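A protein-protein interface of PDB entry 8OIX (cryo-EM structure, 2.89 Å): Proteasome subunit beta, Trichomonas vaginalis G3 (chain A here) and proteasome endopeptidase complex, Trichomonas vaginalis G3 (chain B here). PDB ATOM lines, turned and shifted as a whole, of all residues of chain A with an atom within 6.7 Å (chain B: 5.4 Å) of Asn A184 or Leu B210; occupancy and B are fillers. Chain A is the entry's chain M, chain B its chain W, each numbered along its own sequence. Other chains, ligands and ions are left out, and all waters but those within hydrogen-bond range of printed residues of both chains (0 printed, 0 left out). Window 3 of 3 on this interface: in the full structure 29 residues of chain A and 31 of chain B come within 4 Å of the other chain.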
ATOM      1  N   VAL A  33      -4.659 -12.623 -23.411  1.00  0.00           N
ATOM      2  CA  VAL A  33      -5.120 -11.918 -22.219  1.00  0.00           C
ATOM      3  C   VAL A  33      -4.961 -12.864 -21.038  1.00  0.00           C
ATOM      4  O   VAL A  33      -5.755 -13.797 -20.873  1.00  0.00           O
ATOM      5  CB  VAL A  33      -6.570 -11.447 -22.351  1.00  0.00           C
ATOM      6  CG1 VAL A  33      -6.999 -10.719 -21.096  1.00  0.00           C
ATOM      7  CG2 VAL A  33      -6.726 -10.563 -23.570  1.00  0.00           C
ATOM      8  N   ALA A 163     -17.860 -19.539 -22.037  1.00  0.00           N
ATOM      9  CA  ALA A 163     -17.594 -18.388 -22.891  1.00  0.00           C
ATOM     10  C   ALA A 163     -17.227 -18.802 -24.311  1.00  0.00           C
ATOM     11  O   ALA A 163     -17.541 -18.081 -25.264  1.00  0.00           O
ATOM     12  CB  ALA A 163     -16.481 -17.533 -22.285  1.00  0.00           C
ATOM     13  N   LEU A 179     -10.478  -8.697 -28.513  1.00  0.00           N
ATOM     14  CA  LEU A 179      -9.531  -8.472 -27.425  1.00  0.00           C
ATOM     15  C   LEU A 179     -10.232  -7.948 -26.178  1.00  0.00           C
ATOM     16  O   LEU A 179     -10.010  -8.450 -25.070  1.00  0.00           O
ATOM     17  CB  LEU A 179      -8.445  -7.497 -27.882  1.00  0.00           C
ATOM     18  CG  LEU A 179      -7.596  -6.824 -26.801  1.00  0.00           C
ATOM     19  CD1 LEU A 179      -6.916  -7.861 -25.938  1.00  0.00           C
ATOM     20  CD2 LEU A 179      -6.573  -5.889 -27.424  1.00  0.00           C
ATOM     21  N   GLN A 180     -11.089  -6.940 -26.341  1.00  0.00           N
ATOM     22  CA  GLN A 180     -11.772  -6.374 -25.184  1.00  0.00           C
ATOM     23  C   GLN A 180     -12.749  -7.369 -24.577  1.00  0.00           C
ATOM     24  O   GLN A 180     -12.889  -7.438 -23.352  1.00  0.00           O
ATOM     25  CB  GLN A 180     -12.491  -5.084 -25.569  1.00  0.00           C
ATOM     26  CG  GLN A 180     -13.084  -4.352 -24.381  1.00  0.00           C
ATOM     27  CD  GLN A 180     -12.047  -4.047 -23.320  1.00  0.00           C
ATOM     28  OE1 GLN A 180     -10.953  -3.572 -23.622  1.00  0.00           O
ATOM     29  NE2 GLN A 180     -12.384  -4.325 -22.067  1.00  0.00           N
ATOM     30  N   ASP A 181     -13.428  -8.154 -25.415  1.00  0.00           N
ATOM     31  CA  ASP A 181     -14.333  -9.170 -24.888  1.00  0.00           C
ATOM     32  C   ASP A 181     -13.572 -10.235 -24.111  1.00  0.00           C
ATOM     33  O   ASP A 181     -14.039 -10.698 -23.067  1.00  0.00           O
ATOM     34  CB  ASP A 181     -15.141  -9.803 -26.019  1.00  0.00           C
ATOM     35  CG  ASP A 181     -16.335  -8.963 -26.422  1.00  0.00           C
ATOM     36  OD1 ASP A 181     -16.411  -7.792 -25.997  1.00  0.00           O
ATOM     37  OD2 ASP A 181     -17.199  -9.477 -27.164  1.00  0.00           O
ATOM     38  N   ALA A 182     -12.397 -10.637 -24.599  1.00  0.00           N
ATOM     39  CA  ALA A 182     -11.587 -11.598 -23.855  1.00  0.00           C
ATOM     40  C   ALA A 182     -11.096 -11.011 -22.539  1.00  0.00           C
ATOM     41  O   ALA A 182     -11.047 -11.711 -21.520  1.00  0.00           O
ATOM     42  CB  ALA A 182     -10.411 -12.068 -24.703  1.00  0.00           C
ATOM     43  N   LYS A 183     -10.710  -9.732 -22.541  1.00  0.00           N
ATOM     44  CA  LYS A 183     -10.311  -9.086 -21.294  1.00  0.00           C
ATOM     45  C   LYS A 183     -11.465  -9.064 -20.302  1.00  0.00           C
ATOM     46  O   LYS A 183     -11.276  -9.326 -19.109  1.00  0.00           O
ATOM     47  CB  LYS A 183      -9.817  -7.669 -21.572  1.00  0.00           C
ATOM     48  CG  LYS A 183      -8.507  -7.608 -22.329  1.00  0.00           C
ATOM     49  CD  LYS A 183      -8.213  -6.199 -22.802  1.00  0.00           C
ATOM     50  CE  LYS A 183      -7.844  -5.294 -21.646  1.00  0.00           C
ATOM     51  NZ  LYS A 183      -7.380  -3.964 -22.121  1.00  0.00           N
ATOM     52  N   ASN A 184     -12.670  -8.756 -20.783  1.00  0.00           N
ATOM     53  CA  ASN A 184     -13.845  -8.773 -19.919  1.00  0.00           C
ATOM     54  C   ASN A 184     -14.139 -10.177 -19.408  1.00  0.00           C
ATOM     55  O   ASN A 184     -14.540 -10.351 -18.254  1.00  0.00           O
ATOM     56  CB  ASN A 184     -15.051  -8.208 -20.665  1.00  0.00           C
ATOM     57  CG  ASN A 184     -14.819  -6.802 -21.160  1.00  0.00           C
ATOM     58  OD1 ASN A 184     -13.815  -6.175 -20.827  1.00  0.00           O
ATOM     59  ND2 ASN A 184     -15.746  -6.297 -21.964  1.00  0.00           N
ATOM     60  N   ILE A 185     -13.968 -11.191 -20.260  1.00  0.00           N
ATOM     61  CA  ILE A 185     -14.191 -12.569 -19.830  1.00  0.00           C
ATOM     62  C   ILE A 185     -13.213 -12.943 -18.729  1.00  0.00           C
ATOM     63  O   ILE A 185     -13.592 -13.554 -17.724  1.00  0.00           O
ATOM     64  CB  ILE A 185     -14.083 -13.536 -21.024  1.00  0.00           C
ATOM     65  CG1 ILE A 185     -15.244 -13.336 -21.996  1.00  0.00           C
ATOM     66  CG2 ILE A 185     -14.049 -14.977 -20.543  1.00  0.00           C
ATOM     67  CD1 ILE A 185     -15.009 -13.973 -23.345  1.00  0.00           C
ATOM     68  N   VAL A 186     -11.940 -12.579 -18.895  1.00  0.00           N
ATOM     69  CA  VAL A 186     -10.949 -12.888 -17.871  1.00  0.00           C
ATOM     70  C   VAL A 186     -11.268 -12.144 -16.582  1.00  0.00           C
ATOM     71  O   VAL A 186     -11.167 -12.707 -15.489  1.00  0.00           O
ATOM     72  CB  VAL A 186      -9.529 -12.563 -18.363  1.00  0.00           C
ATOM     73  CG1 VAL A 186      -8.540 -12.778 -17.245  1.00  0.00           C
ATOM     74  CG2 VAL A 186      -9.162 -13.427 -19.542  1.00  0.00           C
ATOM     75  N   ARG A 187     -11.657 -10.872 -16.686  1.00  0.00           N
ATOM     76  CA  ARG A 187     -12.028 -10.109 -15.499  1.00  0.00           C
ATOM     77  C   ARG A 187     -13.198 -10.756 -14.771  1.00  0.00           C
ATOM     78  O   ARG A 187     -13.161 -10.931 -13.550  1.00  0.00           O
ATOM     79  CB  ARG A 187     -12.381  -8.673 -15.882  1.00  0.00           C
ATOM     80  CG  ARG A 187     -11.213  -7.732 -16.033  1.00  0.00           C
ATOM     81  CD  ARG A 187     -11.727  -6.304 -16.076  1.00  0.00           C
ATOM     82  NE  ARG A 187     -12.304  -5.906 -14.798  1.00  0.00           N
ATOM     83  CZ  ARG A 187     -12.901  -4.744 -14.572  1.00  0.00           C
ATOM     84  NH1 ARG A 187     -13.033  -3.837 -15.525  1.00  0.00           N
ATOM     85  NH2 ARG A 187     -13.382  -4.488 -13.358  1.00  0.00           N
ATOM     86  N   ASP A 188     -14.255 -11.102 -15.507  1.00  0.00           N
ATOM     87  CA  ASP A 188     -15.439 -11.687 -14.887  1.00  0.00           C
ATOM     88  C   ASP A 188     -15.123 -13.038 -14.261  1.00  0.00           C
ATOM     89  O   ASP A 188     -15.591 -13.347 -13.158  1.00  0.00           O
ATOM     90  CB  ASP A 188     -16.554 -11.819 -15.924  1.00  0.00           C
ATOM     91  CG  ASP A 188     -17.670 -12.734 -15.467  1.00  0.00           C
ATOM     92  OD1 ASP A 188     -18.581 -12.259 -14.757  1.00  0.00           O
ATOM     93  OD2 ASP A 188     -17.638 -13.931 -15.823  1.00  0.00           O
ATOM     94  N   ALA A 189     -14.329 -13.857 -14.950  1.00  0.00           N
ATOM     95  CA  ALA A 189     -13.957 -15.156 -14.406  1.00  0.00           C
ATOM     96  C   ALA A 189     -13.097 -15.005 -13.157  1.00  0.00           C
ATOM     97  O   ALA A 189     -13.289 -15.734 -12.177  1.00  0.00           O
ATOM     98  CB  ALA A 189     -13.245 -15.978 -15.477  1.00  0.00           C
ATOM     99  N   LEU A 206      -4.284  -7.818 -15.002  1.00  0.00           N
ATOM    100  CA  LEU A 206      -4.770  -8.213 -16.320  1.00  0.00           C
ATOM    101  C   LEU A 206      -3.746  -7.759 -17.353  1.00  0.00           C
ATOM    102  O   LEU A 206      -3.688  -6.580 -17.710  1.00  0.00           O
ATOM    103  CB  LEU A 206      -6.144  -7.609 -16.593  1.00  0.00           C
ATOM    104  CG  LEU A 206      -6.837  -8.091 -17.866  1.00  0.00           C
ATOM    105  CD1 LEU A 206      -7.195  -9.549 -17.720  1.00  0.00           C
ATOM    106  CD2 LEU A 206      -8.075  -7.266 -18.167  1.00  0.00           C
ATOM    107  N   PHE B 208     -17.028  -6.462 -10.784  1.00  0.00           N
ATOM    108  CA  PHE B 208     -17.141  -6.578 -12.228  1.00  0.00           C
ATOM    109  C   PHE B 208     -18.034  -7.756 -12.577  1.00  0.00           C
ATOM    110  O   PHE B 208     -18.078  -8.760 -11.863  1.00  0.00           O
ATOM    111  CB  PHE B 208     -15.776  -6.753 -12.903  1.00  0.00           C
ATOM    112  CG  PHE B 208     -15.853  -6.846 -14.399  1.00  0.00           C
ATOM    113  CD1 PHE B 208     -16.082  -5.718 -15.165  1.00  0.00           C
ATOM    114  CD2 PHE B 208     -15.717  -8.065 -15.036  1.00  0.00           C
ATOM    115  CE1 PHE B 208     -16.159  -5.801 -16.539  1.00  0.00           C
ATOM    116  CE2 PHE B 208     -15.795  -8.155 -16.411  1.00  0.00           C
ATOM    117  CZ  PHE B 208     -16.016  -7.022 -17.163  1.00  0.00           C
ATOM    118  N   ARG B 209     -18.736  -7.620 -13.699  1.00  0.00           N
ATOM    119  CA  ARG B 209     -19.621  -8.660 -14.199  1.00  0.00           C
ATOM    120  C   ARG B 209     -19.984  -8.358 -15.646  1.00  0.00           C
ATOM    121  O   ARG B 209     -20.423  -7.247 -15.958  1.00  0.00           O
ATOM    122  CB  ARG B 209     -20.880  -8.758 -13.336  1.00  0.00           C
ATOM    123  CG  ARG B 209     -21.782  -9.924 -13.682  1.00  0.00           C
ATOM    124  CD  ARG B 209     -22.940 -10.024 -12.708  1.00  0.00           C
ATOM    125  NE  ARG B 209     -22.492 -10.338 -11.357  1.00  0.00           N
ATOM    126  CZ  ARG B 209     -22.354 -11.568 -10.882  1.00  0.00           C
ATOM    127  NH1 ARG B 209     -22.601 -12.630 -11.631  1.00  0.00           N
ATOM    128  NH2 ARG B 209     -21.957 -11.737  -9.624  1.00  0.00           N
ATOM    129  N   LEU B 210     -19.786  -9.329 -16.536  1.00  0.00           N
ATOM    130  CA  LEU B 210     -20.101  -9.145 -17.947  1.00  0.00           C
ATOM    131  C   LEU B 210     -21.569  -8.792 -18.136  1.00  0.00           C
ATOM    132  O   LEU B 210     -22.445  -9.629 -17.895  1.00  0.00           O
ATOM    133  CB  LEU B 210     -19.759 -10.410 -18.735  1.00  0.00           C
ATOM    134  CG  LEU B 210     -18.373 -10.487 -19.370  1.00  0.00           C
ATOM    135  CD1 LEU B 210     -18.090 -11.897 -19.848  1.00  0.00           C
ATOM    136  CD2 LEU B 210     -18.307  -9.517 -20.526  1.00  0.00           C
ATOM    137  N   GLU B 211     -21.854  -7.554 -18.555  1.00  0.00           N
ATOM    138  CA  GLU B 211     -23.242  -7.169 -18.803  1.00  0.00           C
ATOM    139  C   GLU B 211     -23.860  -8.017 -19.910  1.00  0.00           C
ATOM    140  O   GLU B 211     -24.908  -8.643 -19.670  1.00  0.00           O
ATOM    141  CB  GLU B 211     -23.323  -5.662 -19.068  1.00  0.00           C
ATOM    142  CG  GLU B 211     -23.443  -4.815 -17.810  1.00  0.00           C
ATOM    143  CD  GLU B 211     -24.785  -4.981 -17.120  1.00  0.00           C
ATOM    144  OE1 GLU B 211     -25.824  -4.771 -17.780  1.00  0.00           O
ATOM    145  OE2 GLU B 211     -24.800  -5.323 -15.920  1.00  0.00           O
ATOM    146  N   PRO B 212     -23.288  -8.093 -21.132  1.00  0.00           N
ATOM    147  CA  PRO B 212     -23.671  -9.197 -22.021  1.00  0.00           C
ATOM    148  C   PRO B 212     -22.911 -10.463 -21.658  1.00  0.00           C
ATOM    149  O   PRO B 212     -21.722 -10.587 -21.968  1.00  0.00           O
ATOM    150  CB  PRO B 212     -23.292  -8.679 -23.412  1.00  0.00           C
ATOM    151  CG  PRO B 212     -22.148  -7.775 -23.161  1.00  0.00           C
ATOM    152  CD  PRO B 212     -22.389  -7.142 -21.817  1.00  0.00           C
ATOM    153  N   GLN B 213     -23.574 -11.408 -21.000  1.00  0.00           N
ATOM    154  CA  GLN B 213     -22.900 -12.632 -20.585  1.00  0.00           C
ATOM    155  C   GLN B 213     -22.534 -13.458 -21.811  1.00  0.00           C
ATOM    156  O   GLN B 213     -23.414 -13.895 -22.560  1.00  0.00           O
ATOM    157  CB  GLN B 213     -23.787 -13.434 -19.637  1.00  0.00           C
ATOM    158  CG  GLN B 213     -23.148 -14.715 -19.134  1.00  0.00           C
ATOM    159  CD  GLN B 213     -24.136 -15.613 -18.422  1.00  0.00           C
ATOM    160  OE1 GLN B 213     -24.863 -15.171 -17.533  1.00  0.00           O
ATOM    161  NE2 GLN B 213     -24.169 -16.882 -18.810  1.00  0.00           N
ATOM    162  N   ILE B 214     -21.238 -13.672 -22.016  1.00  0.00           N
ATOM    163  CA  ILE B 214     -20.760 -14.420 -23.171  1.00  0.00           C
ATOM    164  C   ILE B 214     -20.843 -15.909 -22.863  1.00  0.00           C
ATOM    165  O   ILE B 214     -20.258 -16.387 -21.886  1.00  0.00           O
ATOM    166  CB  ILE B 214     -19.328 -14.008 -23.542  1.00  0.00           C
ATOM    167  CG1 ILE B 214     -19.250 -12.492 -23.731  1.00  0.00           C
ATOM    168  CG2 ILE B 214     -18.871 -14.734 -24.798  1.00  0.00           C
ATOM    169  CD1 ILE B 214     -17.908 -12.000 -24.213  1.00  0.00           C
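The side-chain amide oxygen (OD1) of Asn A184 lies within hydrogen-bond range of the side-chain amide nitrogen (NE2) of Gln A180 (2.6 Å).
Among the printed residues, merely in contact across the chains: Ala A163 with Ile B214, Asp A181 with Ile B214, Asn A184 with Phe B208, Asn A184 with Leu B210, Ile A185 with Leu B210, Ile A185 with Ile B214, Arg A187 with Phe B208, Asp A188 with Phe B208, Asp A188 with Arg B209 and Asp A188 with Leu B210.
Asn A184 touches just these residues of chain B: Phe B208 (3.1 Å) and Leu B210 (3.5 Å).
Printed residues of chain B within 4 Å of Asp A181: Ile B214 (3.9 Å).
Of the printed residues of chain B, Ala A163 touches Ile B214.
Printed residues of chain B within 4 Å of Ile A185: Leu B210 and Ile B214.
Of the printed residues of chain B, Arg A187 touches Phe B208 (3.3 Å).
Of the printed residues of chain A, Ile B214 touches Ala A163 (3.5 Å), Asp A181 (3.9 Å) and Ile A185 (3.6 Å).
The nearest printed residue of chain B that does not touch Asn A184 is Ile B214 (5.9 Å).
Of the 14 printed residues of chain A, 6 touch a printed residue of chain B.
Of the 7 printed residues of chain B, 4 touch a printed residue of chain A.
Hydrophobic or aromatic side chains of chain B that line the printed part of chain A: Phe B208, Leu B210 and Ile B214.
Among the printed residues, no Asp or Glu carboxylate lies within 4 Å of a Lys or Arg side-chain nitrogen of the other chain.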
